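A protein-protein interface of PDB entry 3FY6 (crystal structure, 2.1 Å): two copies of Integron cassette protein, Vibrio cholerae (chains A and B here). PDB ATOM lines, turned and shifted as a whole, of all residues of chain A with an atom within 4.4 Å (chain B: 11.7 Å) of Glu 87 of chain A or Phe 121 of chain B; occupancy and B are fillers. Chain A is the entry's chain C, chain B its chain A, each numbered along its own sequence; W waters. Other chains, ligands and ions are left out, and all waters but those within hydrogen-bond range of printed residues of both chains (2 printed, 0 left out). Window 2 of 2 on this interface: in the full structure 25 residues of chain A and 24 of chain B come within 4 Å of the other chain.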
ATOM      1  N   HIS A  83     -25.724  -9.371  19.512  1.00  0.00           N
ATOM      2  CA  HIS A  83     -25.983 -10.796  19.395  1.00  0.00           C
ATOM      3  C   HIS A  83     -25.821 -11.533  20.721  1.00  0.00           C
ATOM      4  O   HIS A  83     -26.603 -12.426  21.041  1.00  0.00           O
ATOM      5  CB  HIS A  83     -25.079 -11.433  18.346  1.00  0.00           C
ATOM      6  CG  HIS A  83     -25.285 -12.908  18.193  1.00  0.00           C
ATOM      7  ND1 HIS A  83     -26.450 -13.446  17.691  1.00  0.00           N
ATOM      8  CD2 HIS A  83     -24.473 -13.958  18.467  1.00  0.00           C
ATOM      9  CE1 HIS A  83     -26.349 -14.763  17.662  1.00  0.00           C
ATOM     10  NE2 HIS A  83     -25.159 -15.100  18.126  1.00  0.00           N
ATOM     11  N   ALA A  84     -24.788 -11.175  21.473  1.00  0.00           N
ATOM     12  CA  ALA A  84     -24.539 -11.790  22.771  1.00  0.00           C
ATOM     13  C   ALA A  84     -25.721 -11.523  23.705  1.00  0.00           C
ATOM     14  O   ALA A  84     -26.218 -12.434  24.385  1.00  0.00           O
ATOM     15  CB  ALA A  84     -23.247 -11.250  23.371  1.00  0.00           C
ATOM     16  N   TRP A  85     -26.180 -10.272  23.709  1.00  0.00           N
ATOM     17  CA  TRP A  85     -27.324  -9.858  24.525  1.00  0.00           C
ATOM     18  C   TRP A  85     -28.629 -10.567  24.155  1.00  0.00           C
ATOM     19  O   TRP A  85     -29.356 -11.050  25.026  1.00  0.00           O
ATOM     20  CB  TRP A  85     -27.516  -8.346  24.429  1.00  0.00           C
ATOM     21  CG  TRP A  85     -28.837  -7.855  24.940  1.00  0.00           C
ATOM     22  CD1 TRP A  85     -29.377  -8.081  26.174  1.00  0.00           C
ATOM     23  CD2 TRP A  85     -29.778  -7.032  24.234  1.00  0.00           C
ATOM     24  NE1 TRP A  85     -30.596  -7.456  26.280  1.00  0.00           N
ATOM     25  CE2 TRP A  85     -30.868  -6.804  25.104  1.00  0.00           C
ATOM     26  CE3 TRP A  85     -29.808  -6.471  22.950  1.00  0.00           C
ATOM     27  CZ2 TRP A  85     -31.971  -6.039  24.734  1.00  0.00           C
ATOM     28  CZ3 TRP A  85     -30.909  -5.708  22.582  1.00  0.00           C
ATOM     29  CH2 TRP A  85     -31.975  -5.502  23.472  1.00  0.00           C
ATOM     30  N   LEU A  86     -28.940 -10.600  22.866  1.00  0.00           N
ATOM     31  CA  LEU A  86     -30.169 -11.232  22.402  1.00  0.00           C
ATOM     32  C   LEU A  86     -30.203 -12.735  22.692  1.00  0.00           C
ATOM     33  O   LEU A  86     -31.272 -13.293  22.927  1.00  0.00           O
ATOM     34  CB  LEU A  86     -30.373 -10.977  20.911  1.00  0.00           C
ATOM     35  CG  LEU A  86     -30.789  -9.559  20.530  1.00  0.00           C
ATOM     36  CD1 LEU A  86     -30.895  -9.423  19.004  1.00  0.00           C
ATOM     37  CD2 LEU A  86     -32.106  -9.222  21.196  1.00  0.00           C
ATOM     38  N   GLU A  87     -29.042 -13.388  22.670  1.00  0.00           N
ATOM     39  CA  GLU A  87     -28.969 -14.817  22.977  1.00  0.00           C
ATOM     40  C   GLU A  87     -29.050 -15.068  24.485  1.00  0.00           C
ATOM     41  O   GLU A  87     -29.661 -16.035  24.928  1.00  0.00           O
ATOM     42  CB  GLU A  87     -27.704 -15.448  22.383  1.00  0.00           C
ATOM     43  CG  GLU A  87     -27.686 -15.446  20.869  1.00  0.00           C
ATOM     44  CD  GLU A  87     -28.773 -16.333  20.271  1.00  0.00           C
ATOM     45  OE1 GLU A  87     -28.870 -17.508  20.679  1.00  0.00           O
ATOM     46  OE2 GLU A  87     -29.524 -15.857  19.391  1.00  0.00           O
ATOM     47  N   TRP A  88     -28.446 -14.183  25.269  1.00  0.00           N
ATOM     48  CA  TRP A  88     -28.532 -14.276  26.721  1.00  0.00           C
ATOM     49  C   TRP A  88     -29.984 -14.064  27.141  1.00  0.00           C
ATOM     50  O   TRP A  88     -30.498 -14.720  28.044  1.00  0.00           O
ATOM     51  CB  TRP A  88     -27.617 -13.226  27.360  1.00  0.00           C
ATOM     52  CG  TRP A  88     -27.880 -12.948  28.797  1.00  0.00           C
ATOM     53  CD1 TRP A  88     -27.329 -13.581  29.878  1.00  0.00           C
ATOM     54  CD2 TRP A  88     -28.737 -11.924  29.323  1.00  0.00           C
ATOM     55  NE1 TRP A  88     -27.807 -13.015  31.049  1.00  0.00           N
ATOM     56  CE2 TRP A  88     -28.678 -12.006  30.730  1.00  0.00           C
ATOM     57  CE3 TRP A  88     -29.563 -10.955  28.735  1.00  0.00           C
ATOM     58  CZ2 TRP A  88     -29.404 -11.152  31.558  1.00  0.00           C
ATOM     59  CZ3 TRP A  88     -30.284 -10.111  29.560  1.00  0.00           C
ATOM     60  CH2 TRP A  88     -30.198 -10.214  30.956  1.00  0.00           C
ATOM     61  N   ARG A  89     -30.637 -13.156  26.434  1.00  0.00           N
ATOM     62  CA  ARG A  89     -31.995 -12.730  26.725  1.00  0.00           C
ATOM     63  C   ARG A  89     -33.014 -13.863  26.566  1.00  0.00           C
ATOM     64  O   ARG A  89     -34.018 -13.915  27.274  1.00  0.00           O
ATOM     65  CB  ARG A  89     -32.329 -11.574  25.783  1.00  0.00           C
ATOM     66  CG  ARG A  89     -33.715 -11.075  25.876  1.00  0.00           C
ATOM     67  CD  ARG A  89     -33.935  -9.904  24.936  1.00  0.00           C
ATOM     68  NE  ARG A  89     -35.287  -9.427  25.148  1.00  0.00           N
ATOM     69  CZ  ARG A  89     -36.360 -10.156  24.881  1.00  0.00           C
ATOM     70  NH1 ARG A  89     -36.211 -11.369  24.360  1.00  0.00           N
ATOM     71  NH2 ARG A  89     -37.572  -9.673  25.124  1.00  0.00           N
ATOM     72  N   LYS A  90     -32.767 -14.774  25.634  1.00  0.00           N
ATOM     73  CA  LYS A  90     -33.679 -15.895  25.489  1.00  0.00           C
ATOM     74  C   LYS A  90     -33.216 -17.110  26.274  1.00  0.00           C
ATOM     75  O   LYS A  90     -33.790 -18.184  26.166  1.00  0.00           O
ATOM     76  CB  LYS A  90     -33.943 -16.227  24.025  1.00  0.00           C
ATOM     77  CG  LYS A  90     -32.738 -16.409  23.163  1.00  0.00           C
ATOM     78  CD  LYS A  90     -33.138 -16.121  21.726  1.00  0.00           C
ATOM     79  CE  LYS A  90     -32.416 -17.003  20.737  1.00  0.00           C
ATOM     80  NZ  LYS A  90     -32.717 -16.573  19.346  1.00  0.00           N
ATOM     81  N   GLY A  91     -32.185 -16.918  27.087  1.00  0.00           N
ATOM     82  CA  GLY A  91     -31.704 -17.972  27.958  1.00  0.00           C
ATOM     83  C   GLY A  91     -30.762 -18.982  27.321  1.00  0.00           C
ATOM     84  O   GLY A  91     -30.537 -20.045  27.883  1.00  0.00           O
ATOM     85  N   ALA A  92     -30.198 -18.652  26.164  1.00  0.00           N
ATOM     86  CA  ALA A  92     -29.263 -19.556  25.493  1.00  0.00           C
ATOM     87  C   ALA A  92     -27.890 -19.496  26.144  1.00  0.00           C
ATOM     88  O   ALA A  92     -27.085 -20.416  26.014  1.00  0.00           O
ATOM     89  CB  ALA A  92     -29.157 -19.211  24.008  1.00  0.00           C
ATOM     90  N   LEU A  93     -27.625 -18.389  26.825  1.00  0.00           N
ATOM     91  CA  LEU A  93     -26.384 -18.192  27.559  1.00  0.00           C
ATOM     92  C   LEU A  93     -26.726 -17.788  28.973  1.00  0.00           C
ATOM     93  O   LEU A  93     -27.558 -16.906  29.189  1.00  0.00           O
ATOM     94  CB  LEU A  93     -25.550 -17.065  26.935  1.00  0.00           C
ATOM     95  CG  LEU A  93     -25.349 -17.064  25.416  1.00  0.00           C
ATOM     96  CD1 LEU A  93     -24.610 -15.810  24.981  1.00  0.00           C
ATOM     97  CD2 LEU A  93     -24.603 -18.316  24.973  1.00  0.00           C
ATOM     98  N   GLU A 101     -18.233 -14.832  26.573  1.00  0.00           N
ATOM     99  CA  GLU A 101     -18.300 -14.598  25.135  1.00  0.00           C
ATOM    100  C   GLU A 101     -17.976 -13.137  24.816  1.00  0.00           C
ATOM    101  O   GLU A 101     -17.320 -12.834  23.812  1.00  0.00           O
ATOM    102  CB  GLU A 101     -19.661 -15.002  24.569  1.00  0.00           C
ATOM    103  CG  GLU A 101     -19.993 -16.489  24.727  1.00  0.00           C
ATOM    104  CD  GLU A 101     -19.048 -17.400  23.934  1.00  0.00           C
ATOM    105  OE1 GLU A 101     -18.415 -16.928  22.962  1.00  0.00           O
ATOM    106  OE2 GLU A 101     -18.933 -18.592  24.289  1.00  0.00           O
ATOM    107  N   LYS B 116      -9.975 -13.578  15.021  1.00  0.00           N
ATOM    108  CA  LYS B 116     -11.415 -13.509  15.255  1.00  0.00           C
ATOM    109  C   LYS B 116     -11.869 -14.554  16.284  1.00  0.00           C
ATOM    110  O   LYS B 116     -11.412 -15.685  16.257  1.00  0.00           O
ATOM    111  CB  LYS B 116     -12.160 -13.715  13.939  1.00  0.00           C
ATOM    112  CG  LYS B 116     -13.644 -13.396  13.985  1.00  0.00           C
ATOM    113  CD  LYS B 116     -14.285 -13.551  12.607  1.00  0.00           C
ATOM    114  CE  LYS B 116     -14.407 -15.015  12.208  1.00  0.00           C
ATOM    115  NZ  LYS B 116     -14.957 -15.180  10.828  1.00  0.00           N
ATOM    116  N   PRO B 117     -12.782 -14.175  17.200  1.00  0.00           N
ATOM    117  CA  PRO B 117     -13.271 -15.125  18.206  1.00  0.00           C
ATOM    118  C   PRO B 117     -13.733 -16.441  17.568  1.00  0.00           C
ATOM    119  O   PRO B 117     -14.488 -16.431  16.597  1.00  0.00           O
ATOM    120  CB  PRO B 117     -14.464 -14.394  18.815  1.00  0.00           C
ATOM    121  CG  PRO B 117     -14.129 -12.958  18.667  1.00  0.00           C
ATOM    122  CD  PRO B 117     -13.431 -12.861  17.324  1.00  0.00           C
ATOM    123  N   ASN B 118     -13.291 -17.559  18.126  1.00  0.00           N
ATOM    124  CA  ASN B 118     -13.552 -18.860  17.524  1.00  0.00           C
ATOM    125  C   ASN B 118     -14.267 -19.837  18.458  1.00  0.00           C
ATOM    126  O   ASN B 118     -14.207 -21.047  18.255  1.00  0.00           O
ATOM    127  CB  ASN B 118     -12.241 -19.480  17.035  1.00  0.00           C
ATOM    128  CG  ASN B 118     -12.462 -20.692  16.150  1.00  0.00           C
ATOM    129  OD1 ASN B 118     -13.276 -20.661  15.224  1.00  0.00           O
ATOM    130  ND2 ASN B 118     -11.730 -21.764  16.428  1.00  0.00           N
ATOM    131  N   SER B 119     -14.932 -19.313  19.486  1.00  0.00           N
ATOM    132  CA  SER B 119     -15.794 -20.148  20.318  1.00  0.00           C
ATOM    133  C   SER B 119     -16.937 -20.624  19.437  1.00  0.00           C
ATOM    134  O   SER B 119     -17.269 -19.973  18.439  1.00  0.00           O
ATOM    135  CB  SER B 119     -16.352 -19.359  21.516  1.00  0.00           C
ATOM    136  OG  SER B 119     -17.312 -18.410  21.083  1.00  0.00           O
ATOM    137  N   ASP B 120     -17.528 -21.759  19.795  1.00  0.00           N
ATOM    138  CA  ASP B 120     -18.661 -22.304  19.052  1.00  0.00           C
ATOM    139  C   ASP B 120     -19.794 -21.293  18.971  1.00  0.00           C
ATOM    140  O   ASP B 120     -20.481 -21.192  17.963  1.00  0.00           O
ATOM    141  CB  ASP B 120     -19.146 -23.617  19.682  1.00  0.00           C
ATOM    142  CG  ASP B 120     -18.234 -24.787  19.345  1.00  0.00           C
ATOM    143  OD1 ASP B 120     -17.223 -24.567  18.641  1.00  0.00           O
ATOM    144  OD2 ASP B 120     -18.524 -25.922  19.767  1.00  0.00           O
ATOM    145  N   PHE B 121     -19.982 -20.533  20.036  1.00  0.00           N
ATOM    146  CA  PHE B 121     -20.979 -19.479  20.005  1.00  0.00           C
ATOM    147  C   PHE B 121     -20.704 -18.488  18.878  1.00  0.00           C
ATOM    148  O   PHE B 121     -21.571 -18.227  18.044  1.00  0.00           O
ATOM    149  CB  PHE B 121     -21.028 -18.739  21.333  1.00  0.00           C
ATOM    150  CG  PHE B 121     -22.037 -17.643  21.360  1.00  0.00           C
ATOM    151  CD1 PHE B 121     -23.389 -17.935  21.487  1.00  0.00           C
ATOM    152  CD2 PHE B 121     -21.646 -16.322  21.239  1.00  0.00           C
ATOM    153  CE1 PHE B 121     -24.334 -16.923  21.507  1.00  0.00           C
ATOM    154  CE2 PHE B 121     -22.587 -15.303  21.270  1.00  0.00           C
ATOM    155  CZ  PHE B 121     -23.935 -15.609  21.397  1.00  0.00           C
ATOM    156  N   TRP B 122     -19.500 -17.928  18.842  1.00  0.00           N
ATOM    157  CA  TRP B 122     -19.207 -16.916  17.823  1.00  0.00           C
ATOM    158  C   TRP B 122     -19.170 -17.474  16.384  1.00  0.00           C
ATOM    159  O   TRP B 122     -19.603 -16.804  15.440  1.00  0.00           O
ATOM    160  CB  TRP B 122     -17.945 -16.130  18.167  1.00  0.00           C
ATOM    161  CG  TRP B 122     -18.183 -15.194  19.330  1.00  0.00           C
ATOM    162  CD1 TRP B 122     -17.507 -15.163  20.512  1.00  0.00           C
ATOM    163  CD2 TRP B 122     -19.194 -14.176  19.415  1.00  0.00           C
ATOM    164  NE1 TRP B 122     -18.027 -14.174  21.329  1.00  0.00           N
ATOM    165  CE2 TRP B 122     -19.066 -13.563  20.678  1.00  0.00           C
ATOM    166  CE3 TRP B 122     -20.188 -13.722  18.539  1.00  0.00           C
ATOM    167  CZ2 TRP B 122     -19.904 -12.522  21.093  1.00  0.00           C
ATOM    168  CZ3 TRP B 122     -21.028 -12.697  18.954  1.00  0.00           C
ATOM    169  CH2 TRP B 122     -20.874 -12.103  20.220  1.00  0.00           C
ATOM    170  N   ARG B 123     -18.695 -18.709  16.225  1.00  0.00           N
ATOM    171  CA  ARG B 123     -18.597 -19.325  14.900  1.00  0.00           C
ATOM    172  C   ARG B 123     -19.970 -19.473  14.248  1.00  0.00           C
ATOM    173  O   ARG B 123     -20.109 -19.378  13.031  1.00  0.00           O
ATOM    174  CB  ARG B 123     -17.923 -20.694  15.007  1.00  0.00           C
ATOM    175  CG  ARG B 123     -16.469 -20.636  15.434  1.00  0.00           C
ATOM    176  CD  ARG B 123     -15.972 -21.996  15.909  1.00  0.00           C
ATOM    177  NE  ARG B 123     -16.309 -23.072  14.977  1.00  0.00           N
ATOM    178  CZ  ARG B 123     -15.581 -23.406  13.912  1.00  0.00           C
ATOM    179  NH1 ARG B 123     -14.466 -22.739  13.627  1.00  0.00           N
ATOM    180  NH2 ARG B 123     -15.975 -24.404  13.123  1.00  0.00           N
ATOM    181  N   LYS B 124     -20.982 -19.718  15.067  1.00  0.00           N
ATOM    182  CA  LYS B 124     -22.346 -19.854  14.582  1.00  0.00           C
ATOM    183  C   LYS B 124     -22.846 -18.528  14.025  1.00  0.00           C
ATOM    184  O   LYS B 124     -23.735 -18.485  13.177  1.00  0.00           O
ATOM    185  CB  LYS B 124     -23.269 -20.326  15.710  1.00  0.00           C
ATOM    186  CG  LYS B 124     -24.704 -20.560  15.276  1.00  0.00           C
ATOM    187  CD  LYS B 124     -25.565 -21.064  16.433  1.00  0.00           C
ATOM    188  CE  LYS B 124     -27.018 -21.280  16.013  1.00  0.00           C
ATOM    189  NZ  LYS B 124     -27.200 -22.470  15.130  1.00  0.00           N
ATOM    190  N   TYR B 125     -22.259 -17.440  14.500  1.00  0.00           N
ATOM    191  CA  TYR B 125     -22.743 -16.123  14.138  1.00  0.00           C
ATOM    192  C   TYR B 125     -22.002 -15.522  12.946  1.00  0.00           C
ATOM    193  O   TYR B 125     -22.611 -14.938  12.052  1.00  0.00           O
ATOM    194  CB  TYR B 125     -22.635 -15.181  15.337  1.00  0.00           C
ATOM    195  CG  TYR B 125     -23.325 -13.874  15.088  1.00  0.00           C
ATOM    196  CD1 TYR B 125     -24.702 -13.828  14.947  1.00  0.00           C
ATOM    197  CD2 TYR B 125     -22.609 -12.689  14.971  1.00  0.00           C
ATOM    198  CE1 TYR B 125     -25.351 -12.648  14.716  1.00  0.00           C
ATOM    199  CE2 TYR B 125     -23.259 -11.491  14.736  1.00  0.00           C
ATOM    200  CZ  TYR B 125     -24.634 -11.484  14.612  1.00  0.00           C
ATOM    201  OH  TYR B 125     -25.323 -10.322  14.381  1.00  0.00           O
ATOM    202  N   PHE B 126     -20.685 -15.650  12.941  1.00  0.00           N
ATOM    203  CA  PHE B 126     -19.891 -14.999  11.911  1.00  0.00           C
ATOM    204  C   PHE B 126     -18.489 -15.579  11.875  1.00  0.00           C
ATOM    205  O   PHE B 126     -17.697 -15.253  10.988  1.00  0.00           O
ATOM    206  CB  PHE B 126     -19.850 -13.482  12.135  1.00  0.00           C
ATOM    207  CG  PHE B 126     -18.770 -13.023  13.088  1.00  0.00           C
ATOM    208  CD1 PHE B 126     -18.649 -13.578  14.353  1.00  0.00           C
ATOM    209  CD2 PHE B 126     -17.887 -12.016  12.718  1.00  0.00           C
ATOM    210  CE1 PHE B 126     -17.659 -13.138  15.240  1.00  0.00           C
ATOM    211  CE2 PHE B 126     -16.896 -11.571  13.594  1.00  0.00           C
ATOM    212  CZ  PHE B 126     -16.778 -12.131  14.854  1.00  0.00           C
ATOM    213  OXT PHE B 126     -18.135 -16.394  12.730  1.00  0.00           O
HETATM  214  O   HOH W   1     -19.045 -21.131  22.866  1.00  0.00           O
HETATM  215  O   HOH W   2     -24.308 -17.687  17.989  1.00  0.00           O
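No position is printed for both chains. Of the 8 pairs that touch across the chains among the printed residues, none has its exchanged pair printed and touching as well.
The backbone NH (N) of Trp 122 of chain B is in hydrogen-bond range of the side-chain hydroxyl (OG) of Ser 119 of chain B (3.2 Å). The side-chain carboxylate (OE2) of Glu 87 of chain A lies within salt-bridge range of the side-chain amino group (NZ) of Lys 90 of chain A (3.3 Å). The backbone carbonyl oxygen (O) of Glu 87 of chain A sits at hydrogen-bond distance from the backbone NH (N) of Ala 92 of chain A.
Water W2 bridges a ring nitrogen (NE2) of His 83 of chain A (2.7 Å) and the backbone carbonyl oxygen (O) of Phe 121 of chain B (2.8 Å). Water W1 lies within hydrogen-bond range of the side-chain carboxylate of Glu 101 of chain A, the backbone NH of Phe 121 of chain B and the backbone NH of Asp 120 of chain B.
Among the printed residues, merely in contact across the chains: His 83 of chain A with Tyr 125 of chain B (3.3 Å), His 83 of chain A with Phe 121 of chain B (3.4 Å), Glu 101 of chain A with Phe 121 of chain B (3.5 Å), Leu 93 of chain A with Phe 121 of chain B (3.7 Å), His 83 of chain A with Trp 122 of chain B (3.7 Å) and Glu 87 of chain A with Phe 121 of chain B (3.7 Å).
Of the 11 printed residues of chain B, 4 touch a printed residue of chain A. Of the 12 printed residues of chain A, 4 touch a printed residue of chain B. Hydrophobic or aromatic side chains of chain A within 4 Å of the printed part of chain B: His 83 and Leu 93. Among the printed residues, 8 pairs touch across the chains.
Of the printed residues of chain B, Glu 87 of chain A touches Phe 121 (3.7 Å). Of the printed residues of chain A, Phe 121 of chain B touches His 83, Glu 87, Leu 93 and Glu 101. Of chain B, only Phe 121 (3.4 Å), Trp 122 (3.7 Å) and Tyr 125 (3.3 Å) come within 4 Å of His 83 of chain A. Ala 84 of chain A touches none of the printed residues of chain B. No residue of chain B comes within 4 Å of Gly 91 of chain A. No residue of chain B comes within 4 Å of Ala 92 of chain A. Of chain B, only Ser 119, Phe 121 and Trp 122 come within 4 Å of Glu 101 of chain A. Of the printed residues of chain A, Ser 119 of chain B touches Glu 101. Printed residues of chain A within 4 Å of Trp 122 of chain B: His 83 (3.7 Å) and Glu 101 (2.9 Å). Asn 118 of chain B touches none of the printed residues of chain A. Lys 116 of chain B touches none of the printed residues of chain A. The nearest residue of chain A that does not touch Phe 121 of chain B is Ala 84 of chain A (4.1 Å). The nearest printed residue of chain A that does not touch Tyr 125 of chain B is Glu 87 of chain A (6.8 Å).
OG of Ser 119 of chain B sits at hydrogen-bond distance from OE1 of Glu 101 of chain A (2.6 Å). O of Glu 101 of chain A sits at hydrogen-bond distance from NE1 of Trp 122 of chain B, at 2.9 Å.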
